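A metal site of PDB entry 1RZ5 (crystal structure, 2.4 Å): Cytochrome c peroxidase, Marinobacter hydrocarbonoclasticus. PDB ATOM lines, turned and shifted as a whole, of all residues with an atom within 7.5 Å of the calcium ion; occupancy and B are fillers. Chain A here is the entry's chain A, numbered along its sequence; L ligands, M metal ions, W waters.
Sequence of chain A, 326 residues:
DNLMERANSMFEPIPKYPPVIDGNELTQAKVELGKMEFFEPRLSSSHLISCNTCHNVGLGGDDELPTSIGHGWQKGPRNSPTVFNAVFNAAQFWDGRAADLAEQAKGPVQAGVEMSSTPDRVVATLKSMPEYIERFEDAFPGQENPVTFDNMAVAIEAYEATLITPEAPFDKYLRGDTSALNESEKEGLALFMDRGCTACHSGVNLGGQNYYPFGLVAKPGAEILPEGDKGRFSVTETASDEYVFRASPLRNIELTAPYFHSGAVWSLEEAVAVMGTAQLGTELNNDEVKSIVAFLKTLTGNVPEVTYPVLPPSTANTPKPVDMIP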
ATOM      1  N   ASP A  62       2.985 -19.611  19.640  1.00  0.00           N
ATOM      2  CA  ASP A  62       4.134 -20.072  18.898  1.00  0.00           C
ATOM      3  C   ASP A  62       3.622 -21.014  17.801  1.00  0.00           C
ATOM      4  O   ASP A  62       2.431 -21.002  17.531  1.00  0.00           O
ATOM      5  CB  ASP A  62       5.192 -20.692  19.808  1.00  0.00           C
ATOM      6  CG  ASP A  62       4.707 -21.899  20.518  1.00  0.00           C
ATOM      7  OD1 ASP A  62       3.846 -22.588  19.955  1.00  0.00           O
ATOM      8  OD2 ASP A  62       5.208 -22.188  21.619  1.00  0.00           O
ATOM      9  N   ASP A  63       4.483 -21.800  17.154  1.00  0.00           N
ATOM     10  CA  ASP A  63       4.003 -22.651  16.062  1.00  0.00           C
ATOM     11  C   ASP A  63       4.022 -24.153  16.307  1.00  0.00           C
ATOM     12  O   ASP A  63       3.625 -24.940  15.434  1.00  0.00           O
ATOM     13  CB  ASP A  63       4.792 -22.356  14.786  1.00  0.00           C
ATOM     14  CG  ASP A  63       6.304 -22.558  14.951  1.00  0.00           C
ATOM     15  OD1 ASP A  63       6.729 -23.336  15.856  1.00  0.00           O
ATOM     16  OD2 ASP A  63       7.069 -21.947  14.171  1.00  0.00           O
ATOM     17  N   GLU A  64       4.471 -24.558  17.489  1.00  0.00           N
ATOM     18  CA  GLU A  64       4.553 -25.958  17.878  1.00  0.00           C
ATOM     19  C   GLU A  64       5.396 -26.825  16.939  1.00  0.00           C
ATOM     20  O   GLU A  64       5.143 -28.010  16.797  1.00  0.00           O
ATOM     21  CB  GLU A  64       3.146 -26.554  18.035  1.00  0.00           C
ATOM     22  CG  GLU A  64       3.104 -27.653  19.109  1.00  0.00           C
ATOM     23  CD  GLU A  64       1.733 -28.319  19.270  1.00  0.00           C
ATOM     24  OE1 GLU A  64       1.183 -28.833  18.264  1.00  0.00           O
ATOM     25  OE2 GLU A  64       1.220 -28.347  20.415  1.00  0.00           O
ATOM     26  N   LEU A  65       6.375 -26.221  16.263  1.00  0.00           N
ATOM     27  CA  LEU A  65       7.305 -26.958  15.404  1.00  0.00           C
ATOM     28  C   LEU A  65       8.658 -26.941  16.095  1.00  0.00           C
ATOM     29  O   LEU A  65       8.940 -26.029  16.912  1.00  0.00           O
ATOM     30  CB  LEU A  65       7.505 -26.275  14.052  1.00  0.00           C
ATOM     31  CG  LEU A  65       6.300 -26.001  13.188  1.00  0.00           C
ATOM     32  CD1 LEU A  65       6.789 -25.417  11.899  1.00  0.00           C
ATOM     33  CD2 LEU A  65       5.508 -27.295  12.976  1.00  0.00           C
ATOM     34  N   PRO A  66       9.518 -27.946  15.814  1.00  0.00           N
ATOM     35  CA  PRO A  66      10.847 -27.981  16.438  1.00  0.00           C
ATOM     36  C   PRO A  66      11.521 -26.638  16.117  1.00  0.00           C
ATOM     37  O   PRO A  66      12.058 -25.969  16.998  1.00  0.00           O
ATOM     38  CB  PRO A  66      11.530 -29.151  15.741  1.00  0.00           C
ATOM     39  CG  PRO A  66      10.360 -30.131  15.561  1.00  0.00           C
ATOM     40  CD  PRO A  66       9.221 -29.211  15.099  1.00  0.00           C
ATOM     41  N   ASN A  79      13.651 -22.573  17.366  1.00  0.00           N
ATOM     42  CA  ASN A  79      12.287 -22.793  17.823  1.00  0.00           C
ATOM     43  C   ASN A  79      11.680 -21.392  18.005  1.00  0.00           C
ATOM     44  O   ASN A  79      12.311 -20.497  18.599  1.00  0.00           O
ATOM     45  CB  ASN A  79      12.319 -23.550  19.146  1.00  0.00           C
ATOM     46  CG  ASN A  79      10.923 -23.922  19.664  1.00  0.00           C
ATOM     47  OD1 ASN A  79      10.450 -23.380  20.673  1.00  0.00           O
ATOM     48  ND2 ASN A  79      10.283 -24.883  19.011  1.00  0.00           N
ATOM     49  N   SER A  80      10.490 -21.162  17.461  1.00  0.00           N
ATOM     50  CA  SER A  80       9.870 -19.865  17.667  1.00  0.00           C
ATOM     51  C   SER A  80       9.265 -19.834  19.081  1.00  0.00           C
ATOM     52  O   SER A  80       8.501 -20.717  19.488  1.00  0.00           O
ATOM     53  CB  SER A  80       8.812 -19.592  16.592  1.00  0.00           C
ATOM     54  OG  SER A  80       7.741 -20.499  16.686  1.00  0.00           O
ATOM     55  N   PRO A  81       9.678 -18.846  19.864  1.00  0.00           N
ATOM     56  CA  PRO A  81       9.241 -18.624  21.246  1.00  0.00           C
ATOM     57  C   PRO A  81       7.814 -18.028  21.220  1.00  0.00           C
ATOM     58  O   PRO A  81       7.355 -17.536  20.207  1.00  0.00           O
ATOM     59  CB  PRO A  81      10.296 -17.644  21.771  1.00  0.00           C
ATOM     60  CG  PRO A  81      10.562 -16.822  20.564  1.00  0.00           C
ATOM     61  CD  PRO A  81      10.613 -17.801  19.427  1.00  0.00           C
ATOM     62  N   THR A  82       7.087 -18.096  22.333  1.00  0.00           N
ATOM     63  CA  THR A  82       5.760 -17.539  22.334  1.00  0.00           C
ATOM     64  C   THR A  82       5.817 -16.027  22.376  1.00  0.00           C
ATOM     65  O   THR A  82       6.728 -15.426  22.959  1.00  0.00           O
ATOM     66  CB  THR A  82       4.920 -18.033  23.534  1.00  0.00           C
ATOM     67  OG1 THR A  82       3.625 -17.396  23.496  1.00  0.00           O
ATOM     68  CG2 THR A  82       5.602 -17.690  24.865  1.00  0.00           C
ATOM     69  N   TRP A  94      17.303 -16.220  21.276  1.00  0.00           N
ATOM     70  CA  TRP A  94      17.820 -17.443  21.871  1.00  0.00           C
ATOM     71  C   TRP A  94      19.342 -17.340  22.139  1.00  0.00           C
ATOM     72  O   TRP A  94      19.807 -17.628  23.248  1.00  0.00           O
ATOM     73  CB  TRP A  94      17.598 -18.630  20.922  1.00  0.00           C
ATOM     74  CG  TRP A  94      16.260 -19.268  20.989  1.00  0.00           C
ATOM     75  CD1 TRP A  94      15.297 -19.256  20.027  1.00  0.00           C
ATOM     76  CD2 TRP A  94      15.774 -20.113  22.033  1.00  0.00           C
ATOM     77  NE1 TRP A  94      14.247 -20.041  20.403  1.00  0.00           N
ATOM     78  CE2 TRP A  94      14.508 -20.584  21.630  1.00  0.00           C
ATOM     79  CE3 TRP A  94      16.292 -20.523  23.269  1.00  0.00           C
ATOM     80  CZ2 TRP A  94      13.753 -21.446  22.416  1.00  0.00           C
ATOM     81  CZ3 TRP A  94      15.531 -21.390  24.043  1.00  0.00           C
ATOM     82  CH2 TRP A  94      14.279 -21.838  23.616  1.00  0.00           C
ATOM     83  N   SER A 248      15.162 -19.473  28.914  1.00  0.00           N
ATOM     84  CA  SER A 248      13.780 -19.241  28.525  1.00  0.00           C
ATOM     85  C   SER A 248      12.780 -18.828  29.584  1.00  0.00           C
ATOM     86  O   SER A 248      12.860 -19.229  30.746  1.00  0.00           O
ATOM     87  CB  SER A 248      13.232 -20.477  27.866  1.00  0.00           C
ATOM     88  OG  SER A 248      14.132 -20.952  26.889  1.00  0.00           O
ATOM     89  N   ILE A 253       4.809 -22.483  29.828  1.00  0.00           N
ATOM     90  CA  ILE A 253       5.658 -23.538  29.305  1.00  0.00           C
ATOM     91  C   ILE A 253       4.845 -24.756  28.906  1.00  0.00           C
ATOM     92  O   ILE A 253       5.167 -25.455  27.951  1.00  0.00           O
ATOM     93  CB  ILE A 253       6.762 -23.944  30.347  1.00  0.00           C
ATOM     94  CG1 ILE A 253       7.794 -24.869  29.693  1.00  0.00           C
ATOM     95  CG2 ILE A 253       6.162 -24.640  31.559  1.00  0.00           C
ATOM     96  CD1 ILE A 253       8.788 -24.130  28.846  1.00  0.00           C
ATOM     97  N   LEU A 255       2.221 -24.815  27.428  1.00  0.00           N
ATOM     98  CA  LEU A 255       1.657 -24.645  26.105  1.00  0.00           C
ATOM     99  C   LEU A 255       2.630 -24.277  25.003  1.00  0.00           C
ATOM    100  O   LEU A 255       2.204 -23.955  23.894  1.00  0.00           O
ATOM    101  CB  LEU A 255       0.540 -23.599  26.165  1.00  0.00           C
ATOM    102  CG  LEU A 255      -0.634 -23.961  27.092  1.00  0.00           C
ATOM    103  CD1 LEU A 255      -1.689 -22.862  27.034  1.00  0.00           C
ATOM    104  CD2 LEU A 255      -1.244 -25.277  26.688  1.00  0.00           C
ATOM    105  N   THR A 256       3.936 -24.353  25.263  1.00  0.00           N
ATOM    106  CA  THR A 256       4.886 -23.948  24.232  1.00  0.00           C
ATOM    107  C   THR A 256       5.875 -25.012  23.756  1.00  0.00           C
ATOM    108  O   THR A 256       6.976 -24.691  23.323  1.00  0.00           O
ATOM    109  CB  THR A 256       5.655 -22.680  24.673  1.00  0.00           C
ATOM    110  OG1 THR A 256       6.464 -22.961  25.835  1.00  0.00           O
ATOM    111  CG2 THR A 256       4.635 -21.565  25.026  1.00  0.00           C
ATOM    112  N   ALA A 257       5.461 -26.267  23.835  1.00  0.00           N
ATOM    113  CA  ALA A 257       6.289 -27.379  23.379  1.00  0.00           C
ATOM    114  C   ALA A 257       6.441 -27.219  21.866  1.00  0.00           C
ATOM    115  O   ALA A 257       5.628 -26.568  21.237  1.00  0.00           O
ATOM    116  CB  ALA A 257       5.600 -28.707  23.693  1.00  0.00           C
ATOM    117  N   PRO A 258       7.510 -27.779  21.269  1.00  0.00           N
ATOM    118  CA  PRO A 258       8.620 -28.538  21.886  1.00  0.00           C
ATOM    119  C   PRO A 258       9.610 -27.584  22.536  1.00  0.00           C
ATOM    120  O   PRO A 258       9.554 -26.365  22.318  1.00  0.00           O
ATOM    121  CB  PRO A 258       9.228 -29.286  20.716  1.00  0.00           C
ATOM    122  CG  PRO A 258       8.924 -28.412  19.522  1.00  0.00           C
ATOM    123  CD  PRO A 258       7.510 -27.922  19.801  1.00  0.00           C
ATOM    124  N   TYR A 259      10.537 -28.131  23.302  1.00  0.00           N
ATOM    125  CA  TYR A 259      11.453 -27.312  24.068  1.00  0.00           C
ATOM    126  C   TYR A 259      12.896 -27.126  23.638  1.00  0.00           C
ATOM    127  O   TYR A 259      13.396 -27.843  22.782  1.00  0.00           O
ATOM    128  CB  TYR A 259      11.377 -27.801  25.499  1.00  0.00           C
ATOM    129  CG  TYR A 259       9.942 -27.888  25.976  1.00  0.00           C
ATOM    130  CD1 TYR A 259       9.307 -29.131  26.129  1.00  0.00           C
ATOM    131  CD2 TYR A 259       9.203 -26.719  26.224  1.00  0.00           C
ATOM    132  CE1 TYR A 259       7.942 -29.206  26.509  1.00  0.00           C
ATOM    133  CE2 TYR A 259       7.866 -26.775  26.601  1.00  0.00           C
ATOM    134  CZ  TYR A 259       7.237 -28.010  26.756  1.00  0.00           C
ATOM    135  OH  TYR A 259       5.929 -28.034  27.164  1.00  0.00           O
ATOM    136  N   PHE A 260      13.520 -26.107  24.234  1.00  0.00           N
ATOM    137  CA  PHE A 260      14.904 -25.705  23.992  1.00  0.00           C
ATOM    138  C   PHE A 260      15.030 -25.005  22.652  1.00  0.00           C
ATOM    139  O   PHE A 260      14.107 -25.081  21.824  1.00  0.00           O
ATOM    140  CB  PHE A 260      15.855 -26.909  24.151  1.00  0.00           C
ATOM    141  CG  PHE A 260      15.840 -27.479  25.553  1.00  0.00           C
ATOM    142  CD1 PHE A 260      15.211 -28.673  25.833  1.00  0.00           C
ATOM    143  CD2 PHE A 260      16.332 -26.721  26.610  1.00  0.00           C
ATOM    144  CE1 PHE A 260      15.047 -29.105  27.139  1.00  0.00           C
ATOM    145  CE2 PHE A 260      16.173 -27.150  27.938  1.00  0.00           C
ATOM    146  CZ  PHE A 260      15.524 -28.348  28.195  1.00  0.00           C
ATOM    147  N   HIS A 261      16.155 -24.336  22.447  1.00  0.00           N
ATOM    148  CA  HIS A 261      16.401 -23.540  21.252  1.00  0.00           C
ATOM    149  C   HIS A 261      16.199 -24.273  19.948  1.00  0.00           C
ATOM    150  O   HIS A 261      15.930 -23.663  18.913  1.00  0.00           O
ATOM    151  CB  HIS A 261      17.819 -22.919  21.288  1.00  0.00           C
ATOM    152  CG  HIS A 261      18.910 -23.914  21.044  1.00  0.00           C
ATOM    153  ND1 HIS A 261      19.467 -24.673  22.055  1.00  0.00           N
ATOM    154  CD2 HIS A 261      19.495 -24.316  19.892  1.00  0.00           C
ATOM    155  CE1 HIS A 261      20.344 -25.510  21.529  1.00  0.00           C
ATOM    156  NE2 HIS A 261      20.383 -25.322  20.224  1.00  0.00           N
ATOM    157  N   GLY A 263      13.992 -27.008  19.804  1.00  0.00           N
ATOM    158  CA  GLY A 263      12.720 -27.700  19.829  1.00  0.00           C
ATOM    159  C   GLY A 263      12.934 -29.207  19.700  1.00  0.00           C
ATOM    160  O   GLY A 263      12.104 -29.904  19.127  1.00  0.00           O
ATOM    161  N   VAL A 265      13.115 -31.437  22.237  1.00  0.00           N
ATOM    162  CA  VAL A 265      12.467 -32.183  23.309  1.00  0.00           C
ATOM    163  C   VAL A 265      10.959 -31.882  23.419  1.00  0.00           C
ATOM    164  O   VAL A 265      10.559 -30.755  23.675  1.00  0.00           O
ATOM    165  CB  VAL A 265      13.148 -31.848  24.669  1.00  0.00           C
ATOM    166  CG1 VAL A 265      12.391 -32.487  25.814  1.00  0.00           C
ATOM    167  CG2 VAL A 265      14.610 -32.324  24.645  1.00  0.00           C
HETATM  168 FE1  LIG L   1      16.557 -23.883  32.556  1.00  0.00          FE
HETATM  169  C1  LIG L   1      15.771 -23.848  29.258  1.00  0.00           C
HETATM  170  C2  LIG L   1      13.783 -25.619  33.226  1.00  0.00           C
HETATM  171  C3  LIG L   1      17.648 -24.250  35.773  1.00  0.00           C
HETATM  172  C4  LIG L   1      19.293 -21.986  31.896  1.00  0.00           C
HETATM  173  N1  LIG L   1      14.993 -24.566  31.438  1.00  0.00           N
HETATM  174  C5  LIG L   1      14.845 -24.462  30.080  1.00  0.00           C
HETATM  175  C6  LIG L   1      13.594 -25.097  29.696  1.00  0.00           C
HETATM  176  C7  LIG L   1      13.043 -25.584  30.832  1.00  0.00           C
HETATM  177  C8  LIG L   1      13.926 -25.263  31.919  1.00  0.00           C
HETATM  178  C9  LIG L   1      11.742 -26.391  31.001  1.00  0.00           C
HETATM  179  C10 LIG L   1      13.043 -25.164  28.239  1.00  0.00           C
HETATM  180  C11 LIG L   1      12.299 -23.826  28.003  1.00  0.00           C
HETATM  181  C12 LIG L   1      11.680 -23.617  26.615  1.00  0.00           C
HETATM  182  O1  LIG L   1      10.850 -22.663  26.511  1.00  0.00           O
HETATM  183  O2  LIG L   1      11.967 -24.348  25.681  1.00  0.00           O
HETATM  184  N2  LIG L   1      15.859 -24.739  34.197  1.00  0.00           N
HETATM  185  C13 LIG L   1      14.653 -25.421  34.270  1.00  0.00           C
HETATM  186  C14 LIG L   1      14.473 -25.931  35.616  1.00  0.00           C
HETATM  187  C15 LIG L   1      15.600 -25.601  36.326  1.00  0.00           C
HETATM  188  C16 LIG L   1      16.427 -24.826  35.459  1.00  0.00           C
HETATM  189  C17 LIG L   1      13.245 -26.716  36.075  1.00  0.00           C
HETATM  190  C18 LIG L   1      15.972 -25.943  37.769  1.00  0.00           C
HETATM  191  C19 LIG L   1      16.105 -27.464  38.026  1.00  0.00           C
HETATM  192  N3  LIG L   1      18.149 -23.219  33.619  1.00  0.00           N
HETATM  193  C20 LIG L   1      18.422 -23.467  34.936  1.00  0.00           C
HETATM  194  C21 LIG L   1      19.628 -22.765  35.355  1.00  0.00           C
HETATM  195  C22 LIG L   1      20.079 -22.060  34.293  1.00  0.00           C
HETATM  196  C23 LIG L   1      19.169 -22.381  33.194  1.00  0.00           C
HETATM  197  C24 LIG L   1      20.188 -22.869  36.820  1.00  0.00           C
HETATM  198  C25 LIG L   1      21.290 -21.100  34.170  1.00  0.00           C
HETATM  199  C26 LIG L   1      22.683 -21.709  34.542  1.00  0.00           C
HETATM  200  N4  LIG L   1      17.367 -23.100  30.934  1.00  0.00           N
HETATM  201  C27 LIG L   1      18.518 -22.335  30.828  1.00  0.00           C
HETATM  202  C28 LIG L   1      18.818 -21.994  29.453  1.00  0.00           C
HETATM  203  C29 LIG L   1      17.864 -22.585  28.694  1.00  0.00           C
HETATM  204  C30 LIG L   1      16.938 -23.202  29.619  1.00  0.00           C
HETATM  205  C31 LIG L   1      20.021 -21.154  28.966  1.00  0.00           C
HETATM  206  C32 LIG L   1      17.806 -22.591  27.156  1.00  0.00           C
HETATM  207  C33 LIG L   1      18.663 -23.784  26.628  1.00  0.00           C
HETATM  208  C34 LIG L   1      18.549 -24.056  25.151  1.00  0.00           C
HETATM  209  O3  LIG L   1      17.527 -23.719  24.500  1.00  0.00           O
HETATM  210  O4  LIG L   1      19.485 -24.684  24.612  1.00  0.00           O
HETATM  211 CA    CA M   1       8.972 -23.990  22.470  1.00  0.00          CA
HETATM  212  O   HOH W   1       7.695 -24.528  20.474  1.00  0.00           O
HETATM  213  O   HOH W   2      11.348 -23.830  23.297  1.00  0.00           O
HETATM  214  O   HOH W   3       8.129 -21.894  21.984  1.00  0.00           O
HETATM  215  O   HOH W   4       8.911 -23.363  24.684  1.00  0.00           O
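N of Phe 260 is in hydrogen-bond range of O2 of the ligand, at 2.8 Å.
The backbone NH (N) of His 261 is in hydrogen-bond range of an oxygen (O3) of the ligand, 2.5 Å away.
A ring nitrogen (ND1) of His 261 sits at hydrogen-bond distance from an oxygen (O4) of the ligand, at 2.6 Å.
The indole nitrogen of Trp 94 lies within hydrogen-bond range of the backbone carbonyl oxygen of Asn 79, 2.7 Å away.
The backbone carbonyl oxygen (O) of Pro 66 is in hydrogen-bond range of the side-chain amide nitrogen (ND2) of Asn 79 (2.9 Å).
The backbone NH (N) of Asn 79 lies within hydrogen-bond range of the backbone carbonyl oxygen (O) of His 261 (3.0 Å).
The side-chain amide nitrogen (ND2) of Asn 79 sits at hydrogen-bond distance from the backbone carbonyl oxygen (O) of Leu 65, 2.7 Å away.
Of the 21 residues printed, 3 come within 4 Å of the calcium ion.
The calcium ion is bound by the backbone carbonyl oxygen of Thr 256, water W4, water W3, the side-chain amide oxygen of Asn 79, water W1, the backbone carbonyl oxygen of Pro 258 and water W2.
The calcium ion has seven donor atoms within binding distance.
Water W1 lies within hydrogen-bond range of the side-chain amide nitrogen of Asn 79 and the backbone carbonyl oxygen of Ala 257.
Water W2 lies within hydrogen-bond range of an oxygen (O2) of the ligand (2.5 Å) and the backbone NH of Phe 260 (3.3 Å).
Water W3 bridges the backbone carbonyl oxygen of Ser 80 (2.8 Å) and the side-chain carboxylate of Asp 62 (3.0 Å).
Water W4 bridges the side-chain hydroxyl (OG1) of Thr 256 (2.7 Å) and an oxygen (O1) of the ligand (2.8 Å).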
